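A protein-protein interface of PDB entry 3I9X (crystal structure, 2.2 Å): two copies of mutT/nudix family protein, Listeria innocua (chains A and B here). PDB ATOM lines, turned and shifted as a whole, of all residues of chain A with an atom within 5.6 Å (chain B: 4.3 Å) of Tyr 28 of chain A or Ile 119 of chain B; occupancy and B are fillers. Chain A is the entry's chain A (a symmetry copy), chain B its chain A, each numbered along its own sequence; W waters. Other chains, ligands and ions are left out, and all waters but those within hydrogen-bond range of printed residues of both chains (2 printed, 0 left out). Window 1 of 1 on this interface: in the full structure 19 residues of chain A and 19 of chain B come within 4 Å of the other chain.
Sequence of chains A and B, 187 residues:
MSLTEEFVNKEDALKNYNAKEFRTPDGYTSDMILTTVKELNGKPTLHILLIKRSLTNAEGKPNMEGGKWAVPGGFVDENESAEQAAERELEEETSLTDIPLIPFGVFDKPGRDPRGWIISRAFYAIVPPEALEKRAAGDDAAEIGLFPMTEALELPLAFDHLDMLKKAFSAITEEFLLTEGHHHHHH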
ATOM      1  N   ASP A  26       4.013 -28.089   1.501  1.00  0.00           N
ATOM      2  CA  ASP A  26       5.066 -28.990   1.917  1.00  0.00           C
ATOM      3  C   ASP A  26       6.060 -29.271   0.826  1.00  0.00           C
ATOM      4  O   ASP A  26       7.151 -29.800   1.101  1.00  0.00           O
ATOM      5  CB  ASP A  26       4.427 -30.267   2.424  1.00  0.00           C
ATOM      6  CG  ASP A  26       3.656 -30.018   3.663  1.00  0.00           C
ATOM      7  OD1 ASP A  26       2.506 -30.490   3.807  1.00  0.00           O
ATOM      8  OD2 ASP A  26       4.214 -29.254   4.488  1.00  0.00           O
ATOM      9  N   GLY A  27       5.746 -28.879  -0.407  1.00  0.00           N
ATOM     10  CA  GLY A  27       6.647 -29.225  -1.504  1.00  0.00           C
ATOM     11  C   GLY A  27       6.166 -28.776  -2.863  1.00  0.00           C
ATOM     12  O   GLY A  27       4.984 -28.608  -3.094  1.00  0.00           O
ATOM     13  N   TYR A  28       7.132 -28.605  -3.749  1.00  0.00           N
ATOM     14  CA  TYR A  28       6.901 -28.308  -5.128  1.00  0.00           C
ATOM     15  C   TYR A  28       7.707 -29.306  -5.907  1.00  0.00           C
ATOM     16  O   TYR A  28       8.918 -29.383  -5.707  1.00  0.00           O
ATOM     17  CB  TYR A  28       7.438 -26.892  -5.399  1.00  0.00           C
ATOM     18  CG  TYR A  28       7.182 -26.320  -6.760  1.00  0.00           C
ATOM     19  CD1 TYR A  28       5.961 -26.528  -7.430  1.00  0.00           C
ATOM     20  CD2 TYR A  28       8.116 -25.470  -7.354  1.00  0.00           C
ATOM     21  CE1 TYR A  28       5.725 -25.949  -8.655  1.00  0.00           C
ATOM     22  CE2 TYR A  28       7.879 -24.889  -8.579  1.00  0.00           C
ATOM     23  CZ  TYR A  28       6.684 -25.115  -9.236  1.00  0.00           C
ATOM     24  OH  TYR A  28       6.463 -24.513 -10.482  1.00  0.00           O
ATOM     25  N   THR A  29       7.056 -30.019  -6.832  1.00  0.00           N
ATOM     26  CA  THR A  29       7.741 -30.969  -7.702  1.00  0.00           C
ATOM     27  C   THR A  29       7.610 -30.652  -9.200  1.00  0.00           C
ATOM     28  O   THR A  29       6.707 -29.943  -9.633  1.00  0.00           O
ATOM     29  CB  THR A  29       7.271 -32.414  -7.465  1.00  0.00           C
ATOM     30  OG1 THR A  29       5.903 -32.514  -7.828  1.00  0.00           O
ATOM     31  CG2 THR A  29       7.392 -32.803  -5.999  1.00  0.00           C
ATOM     32  N   SER A  30       8.591 -31.143  -9.947  1.00  0.00           N
ATOM     33  CA  SER A  30       8.650 -31.087 -11.389  1.00  0.00           C
ATOM     34  C   SER A  30       8.536 -32.525 -11.884  1.00  0.00           C
ATOM     35  O   SER A  30       9.438 -33.325 -11.647  1.00  0.00           O
ATOM     36  CB  SER A  30       9.996 -30.526 -11.789  1.00  0.00           C
ATOM     37  OG  SER A  30       9.964 -30.032 -13.100  1.00  0.00           O
ATOM     38  N   GLY A  74      11.168 -34.996  -9.573  1.00  0.00           N
ATOM     39  CA  GLY A  74      11.805 -34.733  -8.281  1.00  0.00           C
ATOM     40  C   GLY A  74      11.340 -33.416  -7.700  1.00  0.00           C
ATOM     41  O   GLY A  74      10.587 -32.654  -8.361  1.00  0.00           O
ATOM     42  N   PHE A  75      11.790 -33.143  -6.464  1.00  0.00           N
ATOM     43  CA  PHE A  75      11.531 -31.856  -5.797  1.00  0.00           C
ATOM     44  C   PHE A  75      12.300 -30.707  -6.427  1.00  0.00           C
ATOM     45  O   PHE A  75      13.429 -30.899  -6.831  1.00  0.00           O
ATOM     46  CB  PHE A  75      11.799 -31.986  -4.292  1.00  0.00           C
ATOM     47  CG  PHE A  75      10.787 -32.851  -3.613  1.00  0.00           C
ATOM     48  CD1 PHE A  75       9.561 -32.332  -3.245  1.00  0.00           C
ATOM     49  CD2 PHE A  75      11.023 -34.201  -3.425  1.00  0.00           C
ATOM     50  CE1 PHE A  75       8.592 -33.128  -2.645  1.00  0.00           C
ATOM     51  CE2 PHE A  75      10.054 -35.011  -2.832  1.00  0.00           C
ATOM     52  CZ  PHE A  75       8.852 -34.467  -2.429  1.00  0.00           C
ATOM     53  N   VAL A  76      11.636 -29.549  -6.600  1.00  0.00           N
ATOM     54  CA  VAL A  76      12.261 -28.336  -7.066  1.00  0.00           C
ATOM     55  C   VAL A  76      12.952 -27.675  -5.848  1.00  0.00           C
ATOM     56  O   VAL A  76      12.429 -27.692  -4.744  1.00  0.00           O
ATOM     57  CB  VAL A  76      11.242 -27.326  -7.702  1.00  0.00           C
ATOM     58  CG1 VAL A  76      11.942 -25.986  -8.104  1.00  0.00           C
ATOM     59  CG2 VAL A  76      10.503 -27.942  -8.939  1.00  0.00           C
ATOM     60  N   GLU A  80      15.787 -22.740  -7.858  1.00  0.00           N
ATOM     61  CA  GLU A  80      15.484 -22.982  -9.280  1.00  0.00           C
ATOM     62  C   GLU A  80      13.967 -22.962  -9.643  1.00  0.00           C
ATOM     63  O   GLU A  80      13.087 -22.994  -8.775  1.00  0.00           O
ATOM     64  CB  GLU A  80      16.104 -24.320  -9.711  1.00  0.00           C
ATOM     65  CG  GLU A  80      15.455 -25.514  -9.043  1.00  0.00           C
ATOM     66  CD  GLU A  80      16.232 -26.829  -9.236  1.00  0.00           C
ATOM     67  OE1 GLU A  80      17.290 -26.848  -9.908  1.00  0.00           O
ATOM     68  OE2 GLU A  80      15.773 -27.828  -8.670  1.00  0.00           O
ATOM     69  N   SER A  81      13.698 -22.872 -10.937  1.00  0.00           N
ATOM     70  CA  SER A  81      12.348 -23.000 -11.458  1.00  0.00           C
ATOM     71  C   SER A  81      12.055 -24.480 -11.678  1.00  0.00           C
ATOM     72  O   SER A  81      12.986 -25.316 -11.728  1.00  0.00           O
ATOM     73  CB  SER A  81      12.234 -22.251 -12.772  1.00  0.00           C
ATOM     74  OG  SER A  81      13.015 -22.902 -13.749  1.00  0.00           O
ATOM     75  N   ALA A  82      10.765 -24.810 -11.785  1.00  0.00           N
ATOM     76  CA  ALA A  82      10.355 -26.184 -12.028  1.00  0.00           C
ATOM     77  C   ALA A  82      10.945 -26.688 -13.365  1.00  0.00           C
ATOM     78  O   ALA A  82      11.296 -27.852 -13.477  1.00  0.00           O
ATOM     79  CB  ALA A  82       8.830 -26.329 -11.999  1.00  0.00           C
ATOM     80  N   ILE A 118       1.539 -31.009  -1.683  1.00  0.00           N
ATOM     81  CA  ILE A 118       2.647 -30.975  -2.668  1.00  0.00           C
ATOM     82  C   ILE A 118       2.054 -30.592  -4.013  1.00  0.00           C
ATOM     83  O   ILE A 118       1.043 -31.153  -4.443  1.00  0.00           O
ATOM     84  CB  ILE A 118       3.457 -32.308  -2.699  1.00  0.00           C
ATOM     85  CG1 ILE A 118       4.148 -32.536  -1.347  1.00  0.00           C
ATOM     86  CG2 ILE A 118       4.538 -32.275  -3.760  1.00  0.00           C
ATOM     87  CD1 ILE A 118       4.461 -33.982  -1.064  1.00  0.00           C
ATOM     88  N   ILE A 119       2.637 -29.567  -4.612  1.00  0.00           N
ATOM     89  CA  ILE A 119       2.163 -29.013  -5.864  1.00  0.00           C
ATOM     90  C   ILE A 119       3.128 -29.487  -6.936  1.00  0.00           C
ATOM     91  O   ILE A 119       4.366 -29.338  -6.783  1.00  0.00           O
ATOM     92  CB  ILE A 119       2.162 -27.489  -5.796  1.00  0.00           C
ATOM     93  CG1 ILE A 119       1.154 -27.013  -4.726  1.00  0.00           C
ATOM     94  CG2 ILE A 119       1.840 -26.870  -7.150  1.00  0.00           C
ATOM     95  CD1 ILE A 119       1.682 -25.793  -3.938  1.00  0.00           C
ATOM     96  N   SER A 120       2.569 -30.135  -7.962  1.00  0.00           N
ATOM     97  CA  SER A 120       3.352 -30.633  -9.081  1.00  0.00           C
ATOM     98  C   SER A 120       3.199 -29.795 -10.341  1.00  0.00           C
ATOM     99  O   SER A 120       2.105 -29.601 -10.808  1.00  0.00           O
ATOM    100  CB  SER A 120       2.942 -32.064  -9.421  1.00  0.00           C
ATOM    101  OG  SER A 120       3.360 -32.365 -10.733  1.00  0.00           O
ATOM    102  N   ARG A 121       4.318 -29.372 -10.907  1.00  0.00           N
ATOM    103  CA  ARG A 121       4.388 -28.769 -12.214  1.00  0.00           C
ATOM    104  C   ARG A 121       4.754 -29.869 -13.226  1.00  0.00           C
ATOM    105  O   ARG A 121       5.809 -30.502 -13.160  1.00  0.00           O
ATOM    106  CB  ARG A 121       5.416 -27.630 -12.173  1.00  0.00           C
ATOM    107  CG  ARG A 121       5.658 -26.800 -13.479  1.00  0.00           C
ATOM    108  CD  ARG A 121       4.468 -26.565 -14.223  1.00  0.00           C
ATOM    109  NE  ARG A 121       4.577 -25.456 -15.155  1.00  0.00           N
ATOM    110  CZ  ARG A 121       3.612 -25.108 -16.010  1.00  0.00           C
ATOM    111  NH1 ARG A 121       2.478 -25.794 -16.068  1.00  0.00           N
ATOM    112  NH2 ARG A 121       3.779 -24.047 -16.805  1.00  0.00           N
ATOM    113  N   PRO B  25       8.139 -24.617   0.322  1.00  0.00           N
ATOM    114  CA  PRO B  25       7.732 -23.289  -0.160  1.00  0.00           C
ATOM    115  C   PRO B  25       6.915 -22.539   0.871  1.00  0.00           C
ATOM    116  O   PRO B  25       6.224 -23.120   1.707  1.00  0.00           O
ATOM    117  CB  PRO B  25       6.871 -23.591  -1.390  1.00  0.00           C
ATOM    118  CG  PRO B  25       7.149 -25.046  -1.721  1.00  0.00           C
ATOM    119  CD  PRO B  25       7.410 -25.680  -0.391  1.00  0.00           C
ATOM    120  N   GLY B  27       4.518 -20.402   0.070  1.00  0.00           N
ATOM    121  CA  GLY B  27       3.179 -20.033  -0.385  1.00  0.00           C
ATOM    122  C   GLY B  27       2.876 -20.438  -1.807  1.00  0.00           C
ATOM    123  O   GLY B  27       3.763 -20.590  -2.625  1.00  0.00           O
ATOM    124  N   TYR B  28       1.589 -20.592  -2.063  1.00  0.00           N
ATOM    125  CA  TYR B  28       1.063 -20.848  -3.369  1.00  0.00           C
ATOM    126  C   TYR B  28      -0.023 -19.834  -3.583  1.00  0.00           C
ATOM    127  O   TYR B  28      -0.951 -19.773  -2.778  1.00  0.00           O
ATOM    128  CB  TYR B  28       0.453 -22.259  -3.360  1.00  0.00           C
ATOM    129  CG  TYR B  28      -0.045 -22.789  -4.669  1.00  0.00           C
ATOM    130  CD1 TYR B  28       0.649 -22.553  -5.872  1.00  0.00           C
ATOM    131  CD2 TYR B  28      -1.158 -23.631  -4.712  1.00  0.00           C
ATOM    132  CE1 TYR B  28       0.206 -23.095  -7.056  1.00  0.00           C
ATOM    133  CE2 TYR B  28      -1.600 -24.173  -5.896  1.00  0.00           C
ATOM    134  CZ  TYR B  28      -0.921 -23.921  -7.075  1.00  0.00           C
ATOM    135  OH  TYR B  28      -1.388 -24.484  -8.269  1.00  0.00           O
ATOM    136  N   THR B  29       0.055 -19.090  -4.691  1.00  0.00           N
ATOM    137  CA  THR B  29      -0.976 -18.120  -5.048  1.00  0.00           C
ATOM    138  C   THR B  29      -1.648 -18.393  -6.403  1.00  0.00           C
ATOM    139  O   THR B  29      -1.109 -19.082  -7.263  1.00  0.00           O
ATOM    140  CB  THR B  29      -0.439 -16.679  -5.050  1.00  0.00           C
ATOM    141  OG1 THR B  29       0.539 -16.558  -6.070  1.00  0.00           O
ATOM    142  CG2 THR B  29       0.226 -16.334  -3.725  1.00  0.00           C
ATOM    143  N   VAL B 106       2.829 -20.790 -14.735  1.00  0.00           N
ATOM    144  CA  VAL B 106       3.291 -20.834 -13.360  1.00  0.00           C
ATOM    145  C   VAL B 106       4.435 -19.807 -13.301  1.00  0.00           C
ATOM    146  O   VAL B 106       5.215 -19.701 -14.225  1.00  0.00           O
ATOM    147  CB  VAL B 106       3.711 -22.257 -12.982  1.00  0.00           C
ATOM    148  CG1 VAL B 106       4.132 -22.324 -11.586  1.00  0.00           C
ATOM    149  CG2 VAL B 106       2.508 -23.205 -13.177  1.00  0.00           C
ATOM    150  N   PHE B 107       4.466 -19.011 -12.255  1.00  0.00           N
ATOM    151  CA  PHE B 107       5.527 -18.056 -12.038  1.00  0.00           C
ATOM    152  C   PHE B 107       6.174 -18.506 -10.766  1.00  0.00           C
ATOM    153  O   PHE B 107       5.560 -18.461  -9.727  1.00  0.00           O
ATOM    154  CB  PHE B 107       4.969 -16.638 -12.002  1.00  0.00           C
ATOM    155  CG  PHE B 107       4.511 -16.208 -13.329  1.00  0.00           C
ATOM    156  CD1 PHE B 107       5.367 -15.514 -14.179  1.00  0.00           C
ATOM    157  CD2 PHE B 107       3.297 -16.643 -13.797  1.00  0.00           C
ATOM    158  CE1 PHE B 107       4.947 -15.192 -15.472  1.00  0.00           C
ATOM    159  CE2 PHE B 107       2.871 -16.337 -15.078  1.00  0.00           C
ATOM    160  CZ  PHE B 107       3.690 -15.603 -15.905  1.00  0.00           C
ATOM    161  N   ASP B 108       7.361 -19.073 -10.913  1.00  0.00           N
ATOM    162  CA  ASP B 108       8.064 -19.724  -9.824  1.00  0.00           C
ATOM    163  C   ASP B 108       9.542 -19.291  -9.727  1.00  0.00           C
ATOM    164  O   ASP B 108      10.260 -19.793  -8.898  1.00  0.00           O
ATOM    165  CB  ASP B 108       7.940 -21.249  -9.965  1.00  0.00           C
ATOM    166  CG  ASP B 108       8.530 -21.776 -11.263  1.00  0.00           C
ATOM    167  OD1 ASP B 108       8.956 -20.978 -12.097  1.00  0.00           O
ATOM    168  OD2 ASP B 108       8.527 -23.009 -11.478  1.00  0.00           O
ATOM    169  N   TRP B 117       9.530 -17.932  -0.728  1.00  0.00           N
ATOM    170  CA  TRP B 117       9.455 -18.859  -1.882  1.00  0.00           C
ATOM    171  C   TRP B 117       7.965 -19.032  -2.233  1.00  0.00           C
ATOM    172  O   TRP B 117       7.257 -19.833  -1.592  1.00  0.00           O
ATOM    173  CB  TRP B 117      10.131 -20.193  -1.511  1.00  0.00           C
ATOM    174  CG  TRP B 117      10.179 -21.245  -2.581  1.00  0.00           C
ATOM    175  CD1 TRP B 117       9.909 -21.092  -3.897  1.00  0.00           C
ATOM    176  CD2 TRP B 117      10.591 -22.606  -2.405  1.00  0.00           C
ATOM    177  NE1 TRP B 117      10.097 -22.287  -4.557  1.00  0.00           N
ATOM    178  CE2 TRP B 117      10.518 -23.229  -3.657  1.00  0.00           C
ATOM    179  CE3 TRP B 117      11.022 -23.351  -1.303  1.00  0.00           C
ATOM    180  CZ2 TRP B 117      10.874 -24.568  -3.849  1.00  0.00           C
ATOM    181  CZ3 TRP B 117      11.362 -24.694  -1.485  1.00  0.00           C
ATOM    182  CH2 TRP B 117      11.286 -25.286  -2.745  1.00  0.00           C
ATOM    183  N   ILE B 118       7.456 -18.203  -3.152  1.00  0.00           N
ATOM    184  CA  ILE B 118       5.997 -18.218  -3.415  1.00  0.00           C
ATOM    185  C   ILE B 118       5.798 -18.557  -4.882  1.00  0.00           C
ATOM    186  O   ILE B 118       6.440 -17.976  -5.760  1.00  0.00           O
ATOM    187  CB  ILE B 118       5.302 -16.892  -2.981  1.00  0.00           C
ATOM    188  CG1 ILE B 118       5.420 -16.707  -1.461  1.00  0.00           C
ATOM    189  CG2 ILE B 118       3.825 -16.902  -3.322  1.00  0.00           C
ATOM    190  CD1 ILE B 118       5.311 -15.273  -1.015  1.00  0.00           C
ATOM    191  N   ILE B 119       4.980 -19.570  -5.117  1.00  0.00           N
ATOM    192  CA  ILE B 119       4.727 -20.084  -6.448  1.00  0.00           C
ATOM    193  C   ILE B 119       3.348 -19.587  -6.844  1.00  0.00           C
ATOM    194  O   ILE B 119       2.370 -19.750  -6.072  1.00  0.00           O
ATOM    195  CB  ILE B 119       4.750 -21.609  -6.434  1.00  0.00           C
ATOM    196  CG1 ILE B 119       6.165 -22.107  -6.062  1.00  0.00           C
ATOM    197  CG2 ILE B 119       4.313 -22.186  -7.774  1.00  0.00           C
ATOM    198  CD1 ILE B 119       6.116 -23.353  -5.149  1.00  0.00           C
ATOM    199  N   SER B 120       3.294 -18.905  -7.993  1.00  0.00           N
ATOM    200  CA  SER B 120       2.046 -18.382  -8.524  1.00  0.00           C
ATOM    201  C   SER B 120       1.512 -19.182  -9.701  1.00  0.00           C
ATOM    202  O   SER B 120       2.199 -19.353 -10.676  1.00  0.00           O
ATOM    203  CB  SER B 120       2.230 -16.939  -8.987  1.00  0.00           C
ATOM    204  OG  SER B 120       1.191 -16.603  -9.878  1.00  0.00           O
ATOM    205  N   ARG B 121       0.259 -19.599  -9.613  1.00  0.00           N
ATOM    206  CA  ARG B 121      -0.489 -20.164 -10.707  1.00  0.00           C
ATOM    207  C   ARG B 121      -1.320 -19.039 -11.348  1.00  0.00           C
ATOM    208  O   ARG B 121      -2.180 -18.416 -10.723  1.00  0.00           O
ATOM    209  CB  ARG B 121      -1.353 -21.311 -10.169  1.00  0.00           C
ATOM    210  CG  ARG B 121      -2.247 -22.106 -11.179  1.00  0.00           C
ATOM    211  CD  ARG B 121      -1.623 -22.310 -12.441  1.00  0.00           C
ATOM    212  NE  ARG B 121      -2.211 -23.393 -13.210  1.00  0.00           N
ATOM    213  CZ  ARG B 121      -1.837 -23.708 -14.452  1.00  0.00           C
ATOM    214  NH1 ARG B 121      -0.895 -23.012 -15.074  1.00  0.00           N
ATOM    215  NH2 ARG B 121      -2.403 -24.747 -15.074  1.00  0.00           N
HETATM  216  O   HOH W   1       9.279 -23.302 -14.346  1.00  0.00           O
HETATM  217  O   HOH W   2      10.824 -22.394  -7.533  1.00  0.00           O
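The backbone NH (N) of Ala 82 of chain A sits at hydrogen-bond distance from the side-chain carboxylate (OD2) of Asp 108 of chain B (2.9 Å). The side-chain carboxylate (OD2) of Asp 108 of chain B sits at hydrogen-bond distance from the side-chain hydroxyl (OH) of Tyr 28 of chain A (2.7 Å).
Tyr 28 of chain A touches Ile 119 of chain B, and with the chains exchanged Ile 119 of chain A touches Tyr 28 of chain B. Positions printed for both chains: 27, 28, 29, 118, 119, 120 and 121. Of the 9 pairs that touch across the chains among the printed residues, 2 have their exchanged pair printed and touching as well.
The backbone NH (N) of Gly 27 of chain B lies within hydrogen-bond range of the backbone carbonyl oxygen (O) of Trp 117 of chain B (3.3 Å). The side-chain hydroxyl (OG) of Ser 30 of chain A sits at hydrogen-bond distance from the backbone carbonyl oxygen (O) of Ala 82 of chain A, 2.6 Å away. O of Thr 29 of chain A lies within hydrogen-bond range of N of Arg 121 of chain A (2.8 Å). The backbone carbonyl oxygen of Gly 27 of chain A lies within hydrogen-bond range of the backbone NH of Ile 119 of chain A (3.0 Å). The backbone NH (N) of Val 76 of chain A lies within hydrogen-bond range of the backbone carbonyl oxygen (O) of Tyr 28 of chain A. The backbone NH (N) of Thr 29 of chain B is in hydrogen-bond range of the backbone carbonyl oxygen (O) of Ile 119 of chain B (2.8 Å).
Water W2 lies within hydrogen-bond range of O of Glu 80 of chain A (2.7 Å), O of Asp 108 of chain B (3.0 Å) and NE1 of Trp 117 of chain B (3.1 Å). Water W1 lies within hydrogen-bond range of the side-chain carboxylate (OD2) of Asp 108 of chain B (3.0 Å) and the backbone NH (N) of Ala 82 of chain A (3.3 Å).
Of the 15 printed residues of chain A, 7 touch a printed residue of chain B. Hydrophobic or aromatic side chains of chain A that line the printed part of chain B: Tyr 28, Ala 82 and Ile 119. Of the 12 printed residues of chain B, 6 touch a printed residue of chain A. Hydrophobic or aromatic side chains of chain B that line the printed part of chain A: Pro 25, Tyr 28, Val 106, Trp 117 and Ile 119. Among the printed residues, no Asp or Glu carboxylate lies within 4 Å of a Lys or Arg side-chain nitrogen of the other chain.
Among the printed residues, merely in contact across the chains: Gly 27 of chain A with Pro 25 of chain B (3.6 Å), Tyr 28 of chain A with Val 106 of chain B (3.4 Å), Tyr 28 of chain A with Ile 119 of chain B (3.5 Å), Val 76 of chain A with Trp 117 of chain B (3.3 Å), Ser 81 of chain A with Asp 108 of chain B (3.6 Å), Ile 119 of chain A with Tyr 28 of chain B (3.5 Å) and Arg 121 of chain A with Val 106 of chain B (3.6 Å).
Of the printed residues of chain B, Gly 27 of chain A touches Pro 25. Tyr 28 of chain A touches just these residues of chain B: Val 106, Asp 108 and Ile 119. Of the printed residues of chain B, Val 76 of chain A touches Trp 117. Of the printed residues of chain A, Pro 25 of chain B touches Gly 27. Printed residues of chain A within 4 Å of Tyr 28 of chain B: Ile 119. Of the printed residues of chain A, Trp 117 of chain B touches Val 76 (3.3 Å). Of chain A, only Tyr 28 comes within 4 Å of Ile 119 of chain B. The nearest residue of chain B that does not touch Tyr 28 of chain A is Pro 25 of chain B (4.1 Å). The nearest residue of chain A that does not touch Ile 119 of chain B is Ile 119 of chain A (5.2 Å). The nearest printed residue of chain A that does not touch Trp 117 of chain B is Tyr 28 of chain A (4.4 Å).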
